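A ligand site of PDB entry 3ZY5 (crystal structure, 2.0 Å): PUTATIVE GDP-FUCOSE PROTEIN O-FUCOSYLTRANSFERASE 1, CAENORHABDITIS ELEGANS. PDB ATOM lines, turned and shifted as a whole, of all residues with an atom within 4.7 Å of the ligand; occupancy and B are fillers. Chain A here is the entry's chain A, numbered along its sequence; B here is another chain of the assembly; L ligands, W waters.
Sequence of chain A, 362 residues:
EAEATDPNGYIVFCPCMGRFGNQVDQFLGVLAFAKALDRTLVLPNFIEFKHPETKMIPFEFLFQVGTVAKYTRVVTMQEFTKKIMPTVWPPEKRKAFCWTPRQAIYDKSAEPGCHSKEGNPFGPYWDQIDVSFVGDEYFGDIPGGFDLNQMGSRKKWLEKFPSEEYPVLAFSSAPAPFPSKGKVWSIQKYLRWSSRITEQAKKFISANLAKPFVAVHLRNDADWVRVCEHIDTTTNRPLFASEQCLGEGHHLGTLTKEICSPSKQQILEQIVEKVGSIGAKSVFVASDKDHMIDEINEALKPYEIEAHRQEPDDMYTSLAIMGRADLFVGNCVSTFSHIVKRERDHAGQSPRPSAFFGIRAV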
ATOM      1  N   GLY A  18      -4.458  -5.995  21.322  1.00  0.00           N
ATOM      2  CA  GLY A  18      -3.861  -7.157  20.659  1.00  0.00           C
ATOM      3  C   GLY A  18      -3.602  -8.376  21.515  1.00  0.00           C
ATOM      4  O   GLY A  18      -3.983  -8.452  22.691  1.00  0.00           O
ATOM      5  N   ARG A  19      -2.952  -9.335  20.893  1.00  0.00           N
ATOM      6  CA  ARG A  19      -2.722 -10.639  21.470  1.00  0.00           C
ATOM      7  C   ARG A  19      -1.393 -10.598  22.233  1.00  0.00           C
ATOM      8  O   ARG A  19      -0.861  -9.521  22.459  1.00  0.00           O
ATOM      9  CB  ARG A  19      -2.775 -11.711  20.357  1.00  0.00           C
ATOM     10  CG  ARG A  19      -4.163 -11.817  19.729  1.00  0.00           C
ATOM     11  CD  ARG A  19      -4.088 -12.018  18.219  1.00  0.00           C
ATOM     12  NE  ARG A  19      -4.272 -13.407  17.853  1.00  0.00           N
ATOM     13  CZ  ARG A  19      -4.239 -13.881  16.604  1.00  0.00           C
ATOM     14  NH1 ARG A  19      -4.009 -13.073  15.565  1.00  0.00           N
ATOM     15  NH2 ARG A  19      -4.425 -15.180  16.403  1.00  0.00           N
ATOM     16  N   PHE A  20      -0.870 -11.759  22.619  1.00  0.00           N
ATOM     17  CA  PHE A  20       0.219 -11.810  23.616  1.00  0.00           C
ATOM     18  C   PHE A  20       1.459 -11.046  23.226  1.00  0.00           C
ATOM     19  O   PHE A  20       2.014 -10.337  24.053  1.00  0.00           O
ATOM     20  CB  PHE A  20       0.573 -13.245  23.970  1.00  0.00           C
ATOM     21  CG  PHE A  20       1.473 -13.374  25.163  1.00  0.00           C
ATOM     22  CD1 PHE A  20       1.062 -12.929  26.434  1.00  0.00           C
ATOM     23  CD2 PHE A  20       2.697 -13.992  25.049  1.00  0.00           C
ATOM     24  CE1 PHE A  20       1.894 -13.080  27.546  1.00  0.00           C
ATOM     25  CE2 PHE A  20       3.521 -14.143  26.138  1.00  0.00           C
ATOM     26  CZ  PHE A  20       3.122 -13.707  27.396  1.00  0.00           C
ATOM     27  N   GLY A  21       1.887 -11.153  21.982  1.00  0.00           N
ATOM     28  CA  GLY A  21       3.010 -10.316  21.472  1.00  0.00           C
ATOM     29  C   GLY A  21       2.852  -8.812  21.647  1.00  0.00           C
ATOM     30  O   GLY A  21       3.739  -8.144  22.191  1.00  0.00           O
ATOM     31  N   ASN A  22       1.717  -8.273  21.181  1.00  0.00           N
ATOM     32  CA  ASN A  22       1.359  -6.879  21.344  1.00  0.00           C
ATOM     33  C   ASN A  22       1.350  -6.519  22.842  1.00  0.00           C
ATOM     34  O   ASN A  22       1.855  -5.465  23.249  1.00  0.00           O
ATOM     35  CB  ASN A  22      -0.023  -6.641  20.712  1.00  0.00           C
ATOM     36  CG  ASN A  22      -0.354  -5.169  20.510  1.00  0.00           C
ATOM     37  OD1 ASN A  22      -1.132  -4.824  19.617  1.00  0.00           O
ATOM     38  ND2 ASN A  22       0.206  -4.304  21.349  1.00  0.00           N
ATOM     39  N   PHE A 178       3.423   1.577  20.965  1.00  0.00           N
ATOM     40  CA  PHE A 178       3.358   0.385  20.153  1.00  0.00           C
ATOM     41  C   PHE A 178       3.509   0.785  18.686  1.00  0.00           C
ATOM     42  O   PHE A 178       2.751   1.643  18.195  1.00  0.00           O
ATOM     43  CB  PHE A 178       2.064  -0.400  20.350  1.00  0.00           C
ATOM     44  CG  PHE A 178       2.041  -1.676  19.561  1.00  0.00           C
ATOM     45  CD1 PHE A 178       2.727  -2.809  20.018  1.00  0.00           C
ATOM     46  CD2 PHE A 178       1.376  -1.739  18.345  1.00  0.00           C
ATOM     47  CE1 PHE A 178       2.753  -4.010  19.252  1.00  0.00           C
ATOM     48  CE2 PHE A 178       1.389  -2.935  17.562  1.00  0.00           C
ATOM     49  CZ  PHE A 178       2.062  -4.059  18.032  1.00  0.00           C
ATOM     50  N   HIS A 217       9.788 -19.813  13.875  1.00  0.00           N
ATOM     51  CA  HIS A 217       8.425 -19.294  14.026  1.00  0.00           C
ATOM     52  C   HIS A 217       7.775 -19.029  12.670  1.00  0.00           C
ATOM     53  O   HIS A 217       8.297 -18.261  11.860  1.00  0.00           O
ATOM     54  CB  HIS A 217       8.427 -18.037  14.903  1.00  0.00           C
ATOM     55  CG  HIS A 217       7.073 -17.382  15.022  1.00  0.00           C
ATOM     56  ND1 HIS A 217       6.892 -16.028  14.864  1.00  0.00           N
ATOM     57  CD2 HIS A 217       5.848 -17.900  15.288  1.00  0.00           C
ATOM     58  CE1 HIS A 217       5.612 -15.739  15.016  1.00  0.00           C
ATOM     59  NE2 HIS A 217       4.956 -16.853  15.282  1.00  0.00           N
ATOM     60  N   ARG A 219       4.517 -17.609  10.867  1.00  0.00           N
ATOM     61  CA  ARG A 219       3.311 -16.803  10.998  1.00  0.00           C
ATOM     62  C   ARG A 219       2.660 -16.711   9.615  1.00  0.00           C
ATOM     63  O   ARG A 219       3.235 -16.117   8.688  1.00  0.00           O
ATOM     64  CB  ARG A 219       3.684 -15.423  11.568  1.00  0.00           C
ATOM     65  CG  ARG A 219       2.516 -14.538  11.958  1.00  0.00           C
ATOM     66  CD  ARG A 219       2.028 -14.726  13.401  1.00  0.00           C
ATOM     67  NE  ARG A 219       1.257 -13.556  13.811  1.00  0.00           N
ATOM     68  CZ  ARG A 219      -0.012 -13.318  13.478  1.00  0.00           C
ATOM     69  NH1 ARG A 219      -0.670 -14.194  12.726  1.00  0.00           N
ATOM     70  NH2 ARG A 219      -0.614 -12.216  13.896  1.00  0.00           N
ATOM     71  N   TRP A 224      -2.602 -12.270   8.465  1.00  0.00           N
ATOM     72  CA  TRP A 224      -1.200 -11.874   8.414  1.00  0.00           C
ATOM     73  C   TRP A 224      -0.712 -11.599   6.985  1.00  0.00           C
ATOM     74  O   TRP A 224      -0.023 -10.605   6.745  1.00  0.00           O
ATOM     75  CB  TRP A 224      -0.333 -12.949   9.078  1.00  0.00           C
ATOM     76  CG  TRP A 224       1.111 -12.629   9.125  1.00  0.00           C
ATOM     77  CD1 TRP A 224       2.085 -13.110   8.290  1.00  0.00           C
ATOM     78  CD2 TRP A 224       1.786 -11.766  10.060  1.00  0.00           C
ATOM     79  NE1 TRP A 224       3.313 -12.608   8.639  1.00  0.00           N
ATOM     80  CE2 TRP A 224       3.162 -11.774   9.723  1.00  0.00           C
ATOM     81  CE3 TRP A 224       1.357 -10.988  11.141  1.00  0.00           C
ATOM     82  CZ2 TRP A 224       4.110 -11.026  10.437  1.00  0.00           C
ATOM     83  CZ3 TRP A 224       2.291 -10.253  11.851  1.00  0.00           C
ATOM     84  CH2 TRP A 224       3.661 -10.278  11.490  1.00  0.00           C
ATOM     85  N   VAL A 227      -1.899  -8.170   5.807  1.00  0.00           N
ATOM     86  CA  VAL A 227      -1.141  -6.977   6.239  1.00  0.00           C
ATOM     87  C   VAL A 227       0.217  -6.878   5.551  1.00  0.00           C
ATOM     88  O   VAL A 227       0.726  -5.776   5.312  1.00  0.00           O
ATOM     89  CB  VAL A 227      -0.952  -6.852   7.790  1.00  0.00           C
ATOM     90  CG1 VAL A 227      -2.305  -6.999   8.518  1.00  0.00           C
ATOM     91  CG2 VAL A 227       0.076  -7.837   8.319  1.00  0.00           C
ATOM     92  N   PHE A 240       5.035  -3.131  12.739  1.00  0.00           N
ATOM     93  CA  PHE A 240       5.108  -3.896  13.987  1.00  0.00           C
ATOM     94  C   PHE A 240       6.549  -4.040  14.493  1.00  0.00           C
ATOM     95  O   PHE A 240       7.182  -3.039  14.857  1.00  0.00           O
ATOM     96  CB  PHE A 240       4.337  -5.213  13.826  1.00  0.00           C
ATOM     97  CG  PHE A 240       2.903  -4.979  13.401  1.00  0.00           C
ATOM     98  CD1 PHE A 240       2.093  -4.120  14.136  1.00  0.00           C
ATOM     99  CD2 PHE A 240       2.396  -5.568  12.245  1.00  0.00           C
ATOM    100  CE1 PHE A 240       0.762  -3.868  13.733  1.00  0.00           C
ATOM    101  CE2 PHE A 240       1.080  -5.332  11.836  1.00  0.00           C
ATOM    102  CZ  PHE A 240       0.260  -4.480  12.583  1.00  0.00           C
ATOM    103  N   ALA A 286       6.997 -23.549  15.797  1.00  0.00           N
ATOM    104  CA  ALA A 286       5.832 -22.898  16.352  1.00  0.00           C
ATOM    105  C   ALA A 286       5.179 -22.109  15.241  1.00  0.00           C
ATOM    106  O   ALA A 286       5.850 -21.463  14.446  1.00  0.00           O
ATOM    107  CB  ALA A 286       6.203 -21.987  17.495  1.00  0.00           C
ATOM    108  N   SER A 287       3.853 -22.176  15.178  1.00  0.00           N
ATOM    109  CA  SER A 287       3.079 -21.481  14.166  1.00  0.00           C
ATOM    110  C   SER A 287       1.695 -21.111  14.693  1.00  0.00           C
ATOM    111  O   SER A 287       1.153 -21.753  15.609  1.00  0.00           O
ATOM    112  CB  SER A 287       2.926 -22.373  12.916  1.00  0.00           C
ATOM    113  OG  SER A 287       2.031 -21.796  11.987  1.00  0.00           O
ATOM    114  N   ASP A 288       1.134 -20.062  14.104  1.00  0.00           N
ATOM    115  CA  ASP A 288      -0.230 -19.643  14.393  1.00  0.00           C
ATOM    116  C   ASP A 288      -1.268 -20.525  13.695  1.00  0.00           C
ATOM    117  O   ASP A 288      -2.469 -20.442  14.000  1.00  0.00           O
ATOM    118  CB  ASP A 288      -0.410 -18.188  13.938  1.00  0.00           C
ATOM    119  CG  ASP A 288      -0.174 -17.981  12.445  1.00  0.00           C
ATOM    120  OD1 ASP A 288       0.482 -18.833  11.795  1.00  0.00           O
ATOM    121  OD2 ASP A 288      -0.644 -16.958  11.916  1.00  0.00           O
ATOM    122  N   ASP A 313      -1.005 -26.825  20.486  1.00  0.00           N
ATOM    123  CA  ASP A 313       0.089 -25.850  20.443  1.00  0.00           C
ATOM    124  C   ASP A 313       0.010 -24.696  21.463  1.00  0.00           C
ATOM    125  O   ASP A 313      -0.609 -23.652  21.215  1.00  0.00           O
ATOM    126  CB  ASP A 313       0.295 -25.323  19.010  1.00  0.00           C
ATOM    127  CG  ASP A 313       1.704 -24.779  18.791  1.00  0.00           C
ATOM    128  OD1 ASP A 313       2.576 -25.036  19.643  1.00  0.00           O
ATOM    129  OD2 ASP A 313       1.950 -24.126  17.758  1.00  0.00           O
ATOM    130  N   ASP A 314       0.698 -24.887  22.579  1.00  0.00           N
ATOM    131  CA  ASP A 314       0.779 -23.958  23.716  1.00  0.00           C
ATOM    132  C   ASP A 314       1.715 -22.767  23.374  1.00  0.00           C
ATOM    133  O   ASP A 314       2.930 -22.927  23.283  1.00  0.00           O
ATOM    134  CB  ASP A 314       1.310 -24.771  24.902  1.00  0.00           C
ATOM    135  CG  ASP A 314       1.346 -24.013  26.220  1.00  0.00           C
ATOM    136  OD1 ASP A 314       1.513 -22.785  26.268  1.00  0.00           O
ATOM    137  OD2 ASP A 314       1.281 -24.696  27.244  1.00  0.00           O
ATOM    138  N   MET A 315       1.154 -21.583  23.156  1.00  0.00           N
ATOM    139  CA  MET A 315       1.961 -20.464  22.667  1.00  0.00           C
ATOM    140  C   MET A 315       3.064 -20.088  23.654  1.00  0.00           C
ATOM    141  O   MET A 315       4.162 -19.754  23.249  1.00  0.00           O
ATOM    142  CB  MET A 315       1.098 -19.236  22.347  1.00  0.00           C
ATOM    143  CG  MET A 315       0.555 -18.514  23.583  1.00  0.00           C
ATOM    144  SD  MET A 315      -0.616 -17.218  23.155  1.00  0.00           S
ATOM    145  CE  MET A 315       0.500 -15.967  22.608  1.00  0.00           C
ATOM    146  N   VAL A 333       8.729  -9.267  11.284  1.00  0.00           N
ATOM    147  CA  VAL A 333       7.596  -8.373  11.465  1.00  0.00           C
ATOM    148  C   VAL A 333       6.842  -8.680  12.759  1.00  0.00           C
ATOM    149  O   VAL A 333       6.257  -7.794  13.389  1.00  0.00           O
ATOM    150  CB  VAL A 333       6.671  -8.396  10.206  1.00  0.00           C
ATOM    151  CG1 VAL A 333       5.504  -7.409  10.300  1.00  0.00           C
ATOM    152  CG2 VAL A 333       7.503  -8.071   8.972  1.00  0.00           C
ATOM    153  N   SER A 334       6.863  -9.948  13.173  1.00  0.00           N
ATOM    154  CA  SER A 334       6.034 -10.394  14.297  1.00  0.00           C
ATOM    155  C   SER A 334       6.575 -10.034  15.690  1.00  0.00           C
ATOM    156  O   SER A 334       7.769 -10.220  15.976  1.00  0.00           O
ATOM    157  CB  SER A 334       5.769 -11.898  14.160  1.00  0.00           C
ATOM    158  OG  SER A 334       5.131 -12.399  15.319  1.00  0.00           O
ATOM    159  N   THR A 335       5.700  -9.484  16.535  1.00  0.00           N
ATOM    160  CA  THR A 335       6.032  -9.148  17.920  1.00  0.00           C
ATOM    161  C   THR A 335       6.133 -10.421  18.777  1.00  0.00           C
ATOM    162  O   THR A 335       6.738 -10.399  19.841  1.00  0.00           O
ATOM    163  CB  THR A 335       5.038  -8.149  18.563  1.00  0.00           C
ATOM    164  OG1 THR A 335       3.727  -8.726  18.634  1.00  0.00           O
ATOM    165  CG2 THR A 335       4.943  -6.865  17.752  1.00  0.00           C
ATOM    166  N   PHE A 336       5.516 -11.496  18.295  1.00  0.00           N
ATOM    167  CA  PHE A 336       5.653 -12.812  18.903  1.00  0.00           C
ATOM    168  C   PHE A 336       7.107 -13.303  18.786  1.00  0.00           C
ATOM    169  O   PHE A 336       7.743 -13.647  19.795  1.00  0.00           O
ATOM    170  CB  PHE A 336       4.680 -13.779  18.204  1.00  0.00           C
ATOM    171  CG  PHE A 336       4.389 -15.026  18.998  1.00  0.00           C
ATOM    172  CD1 PHE A 336       3.484 -15.007  20.060  1.00  0.00           C
ATOM    173  CD2 PHE A 336       4.997 -16.218  18.654  1.00  0.00           C
ATOM    174  CE1 PHE A 336       3.224 -16.160  20.780  1.00  0.00           C
ATOM    175  CE2 PHE A 336       4.725 -17.383  19.356  1.00  0.00           C
ATOM    176  CZ  PHE A 336       3.835 -17.351  20.422  1.00  0.00           C
ATOM    177  N   ALA B 110      -8.552  -4.257  12.524  1.00  0.00           N
ATOM    178  CA  ALA B 110      -7.958  -5.264  13.412  1.00  0.00           C
ATOM    179  C   ALA B 110      -6.465  -5.032  13.731  1.00  0.00           C
ATOM    180  O   ALA B 110      -5.958  -5.474  14.785  1.00  0.00           O
ATOM    181  CB  ALA B 110      -8.175  -6.666  12.851  1.00  0.00           C
ATOM    182  N   GLU B 111      -5.731  -4.420  12.816  1.00  0.00           N
ATOM    183  CA  GLU B 111      -4.411  -3.930  13.167  1.00  0.00           C
ATOM    184  C   GLU B 111      -4.624  -2.717  14.077  1.00  0.00           C
ATOM    185  O   GLU B 111      -5.624  -1.997  13.933  1.00  0.00           O
ATOM    186  CB  GLU B 111      -3.564  -3.593  11.938  1.00  0.00           C
ATOM    187  CG  GLU B 111      -4.154  -2.564  10.958  1.00  0.00           C
ATOM    188  CD  GLU B 111      -3.912  -2.962   9.489  1.00  0.00           C
ATOM    189  OE1 GLU B 111      -3.020  -3.811   9.234  1.00  0.00           O
ATOM    190  OE2 GLU B 111      -4.611  -2.416   8.598  1.00  0.00           O
ATOM    191  N   PRO B 112      -3.712  -2.502  15.036  1.00  0.00           N
ATOM    192  CA  PRO B 112      -3.931  -1.321  15.870  1.00  0.00           C
ATOM    193  C   PRO B 112      -4.003  -0.069  15.025  1.00  0.00           C
ATOM    194  O   PRO B 112      -3.293   0.050  14.019  1.00  0.00           O
ATOM    195  CB  PRO B 112      -2.712  -1.324  16.781  1.00  0.00           C
ATOM    196  CG  PRO B 112      -2.441  -2.791  16.986  1.00  0.00           C
ATOM    197  CD  PRO B 112      -2.654  -3.375  15.586  1.00  0.00           C
HETATM  198  O1  LIG L   1       1.148 -12.352  19.586  1.00  0.00           O
HETATM  199  P1  LIG L   1       0.740 -11.350  18.533  1.00  0.00           P
HETATM  200  O2  LIG L   1       0.283 -10.007  19.034  1.00  0.00           O
HETATM  201  O3  LIG L   1       2.029 -11.193  17.546  1.00  0.00           O
HETATM  202  O4  LIG L   1      -0.346 -12.011  17.573  1.00  0.00           O
HETATM  203  P2  LIG L   1       2.174 -10.623  16.039  1.00  0.00           P
HETATM  204  C1  LIG L   1      -0.074 -13.324  17.095  1.00  0.00           C
HETATM  205  C2  LIG L   1      -0.973 -14.253  17.903  1.00  0.00           C
HETATM  206  O5  LIG L   1      -1.351 -15.372  17.083  1.00  0.00           O
HETATM  207  C3  LIG L   1      -0.286 -14.840  19.129  1.00  0.00           C
HETATM  208  C4  LIG L   1      -1.087 -16.606  17.766  1.00  0.00           C
HETATM  209  O6  LIG L   1      -0.471 -14.044  20.319  1.00  0.00           O
HETATM  210  C5  LIG L   1      -0.903 -16.221  19.226  1.00  0.00           C
HETATM  211  O7  LIG L   1      -2.176 -16.192  19.882  1.00  0.00           O
HETATM  212  N1  LIG L   1       0.227 -17.176  17.355  1.00  0.00           N
HETATM  213  C6  LIG L   1       1.184 -16.648  16.559  1.00  0.00           C
HETATM  214  C7  LIG L   1       0.656 -18.346  17.816  1.00  0.00           C
HETATM  215  N2  LIG L   1       2.233 -17.506  16.523  1.00  0.00           N
HETATM  216  C8  LIG L   1       1.913 -18.574  17.280  1.00  0.00           C
HETATM  217  C9  LIG L   1       2.553 -19.760  17.623  1.00  0.00           C
HETATM  218  O8  LIG L   1       3.696 -19.987  17.151  1.00  0.00           O
HETATM  219  N3  LIG L   1       1.945 -20.627  18.473  1.00  0.00           N
HETATM  220  C10 LIG L   1       0.723 -20.353  18.975  1.00  0.00           C
HETATM  221  N4  LIG L   1       0.065 -21.191  19.803  1.00  0.00           N
HETATM  222  N5  LIG L   1       0.076 -19.227  18.656  1.00  0.00           N
HETATM  223  C11 LIG L   1       0.373  -8.844  15.243  1.00  0.00           C
HETATM  224  C12 LIG L   1      -0.453  -8.238  16.391  1.00  0.00           C
HETATM  225  O9  LIG L   1       0.697 -10.162  15.621  1.00  0.00           O
HETATM  226  O10 LIG L   1      -0.401  -9.009  14.063  1.00  0.00           O
HETATM  227  C13 LIG L   1      -1.178  -6.950  16.017  1.00  0.00           C
HETATM  228  O11 LIG L   1       0.403  -7.961  17.502  1.00  0.00           O
HETATM  229  C14 LIG L   1      -1.922  -7.152  14.688  1.00  0.00           C
HETATM  230  O12 LIG L   1      -2.088  -6.560  17.075  1.00  0.00           O
HETATM  231  C15 LIG L   1      -1.067  -7.821  13.599  1.00  0.00           C
HETATM  232  O13 LIG L   1      -3.066  -7.979  14.934  1.00  0.00           O
HETATM  233  C16 LIG L   1      -1.942  -8.207  12.412  1.00  0.00           C
HETATM  234  O14 LIG L   1       3.152  -9.474  16.101  1.00  0.00           O
HETATM  235  O15 LIG L   1       2.533 -11.766  15.120  1.00  0.00           O
HETATM  236  O   HOH W   1      -3.521  -8.541  17.731  1.00  0.00           O
HETATM  237  O   HOH W   2      -3.208 -10.654  15.014  1.00  0.00           O
HETATM  238  O   HOH W   3      -2.495 -14.359  22.332  1.00  0.00           O
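Water W1 bridges O12 of the ligand (2.5 Å) and N of Arg 19 (3.3 Å). Water W2 lies within hydrogen-bond range of the guanidinium group (NH1) of Arg 19 (2.6 Å), an oxygen (O13) of the ligand (2.7 Å) and the guanidinium group (NH2) of Arg 219 (3.2 Å). Water W3 lies within hydrogen-bond range of an oxygen (O6) of the ligand (2.9 Å), the backbone NH of Phe 20 (3.1 Å) and the side-chain sulfur of Met 315 (3.5 Å).
O15 of the ligand lies within salt-bridge range of NE of Arg 219 (2.6 Å). The backbone NH of Thr 335 sits at hydrogen-bond distance from an oxygen (O14) of the ligand, 2.6 Å away. An oxygen (O14) of the ligand lies within hydrogen-bond range of the side-chain hydroxyl (OG1) of Thr 335 (2.7 Å). OG of Ser 334 lies within hydrogen-bond range of O15 of the ligand (2.7 Å). An oxygen (O1) of the ligand sits at hydrogen-bond distance from the backbone NH (N) of Gly 21 (2.8 Å). The backbone carbonyl oxygen (O) of Asp 313 is in hydrogen-bond range of a nitrogen (N4) of the ligand (2.9 Å). The backbone NH (N) of Ser 287 sits at hydrogen-bond distance from an oxygen (O8) of the ligand, at 3.0 Å. O of Ser 287 lies close to N3 of the ligand. NE2 of His 217 sits at hydrogen-bond distance from N2 of the ligand (3.1 Å). An oxygen (O2) of the ligand sits at hydrogen-bond distance from the backbone NH (N) of Asn 22, at 3.1 Å. OD1 of Asn 22 sits at hydrogen-bond distance from O12 of the ligand (3.2 Å). SD of Met 315 sits at hydrogen-bond distance from O7 of the ligand. The guanidinium group (NH2) of Arg 19 is in hydrogen-bond range of an oxygen (O5) of the ligand (3.2 Å). O6 of the ligand sits at hydrogen-bond distance from N of Phe 20 (3.3 Å).
Merely in contact with the ligand: Trp 224 (3.6 Å), Phe 240 (3.7 Å), Ala 286 (3.2 Å), Asp 288 (3.4 Å), Phe 336 (3.6 Å), Ala 110 of chain B (3.8 Å) and Pro 112 of chain B (3.6 Å). Hydrophobic or aromatic side chains that line the ligand: Phe 20, His 217, Trp 224, Phe 240, Ala 286, Met 315, Phe 336 and Pro 112 of chain B. Of the 24 residues printed, 18 come within 4 Å of the ligand.
NH1 of Arg 219 lies within salt-bridge range of OD2 of Asp 288, at 2.9 Å. OG1 of Thr 335 is in hydrogen-bond range of N of Asn 22. OG of Ser 334 is in hydrogen-bond range of N of Phe 336, at 3.1 Å. OD1 of Asp 288 sits at hydrogen-bond distance from OG of Ser 287, 3.3 Å away.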
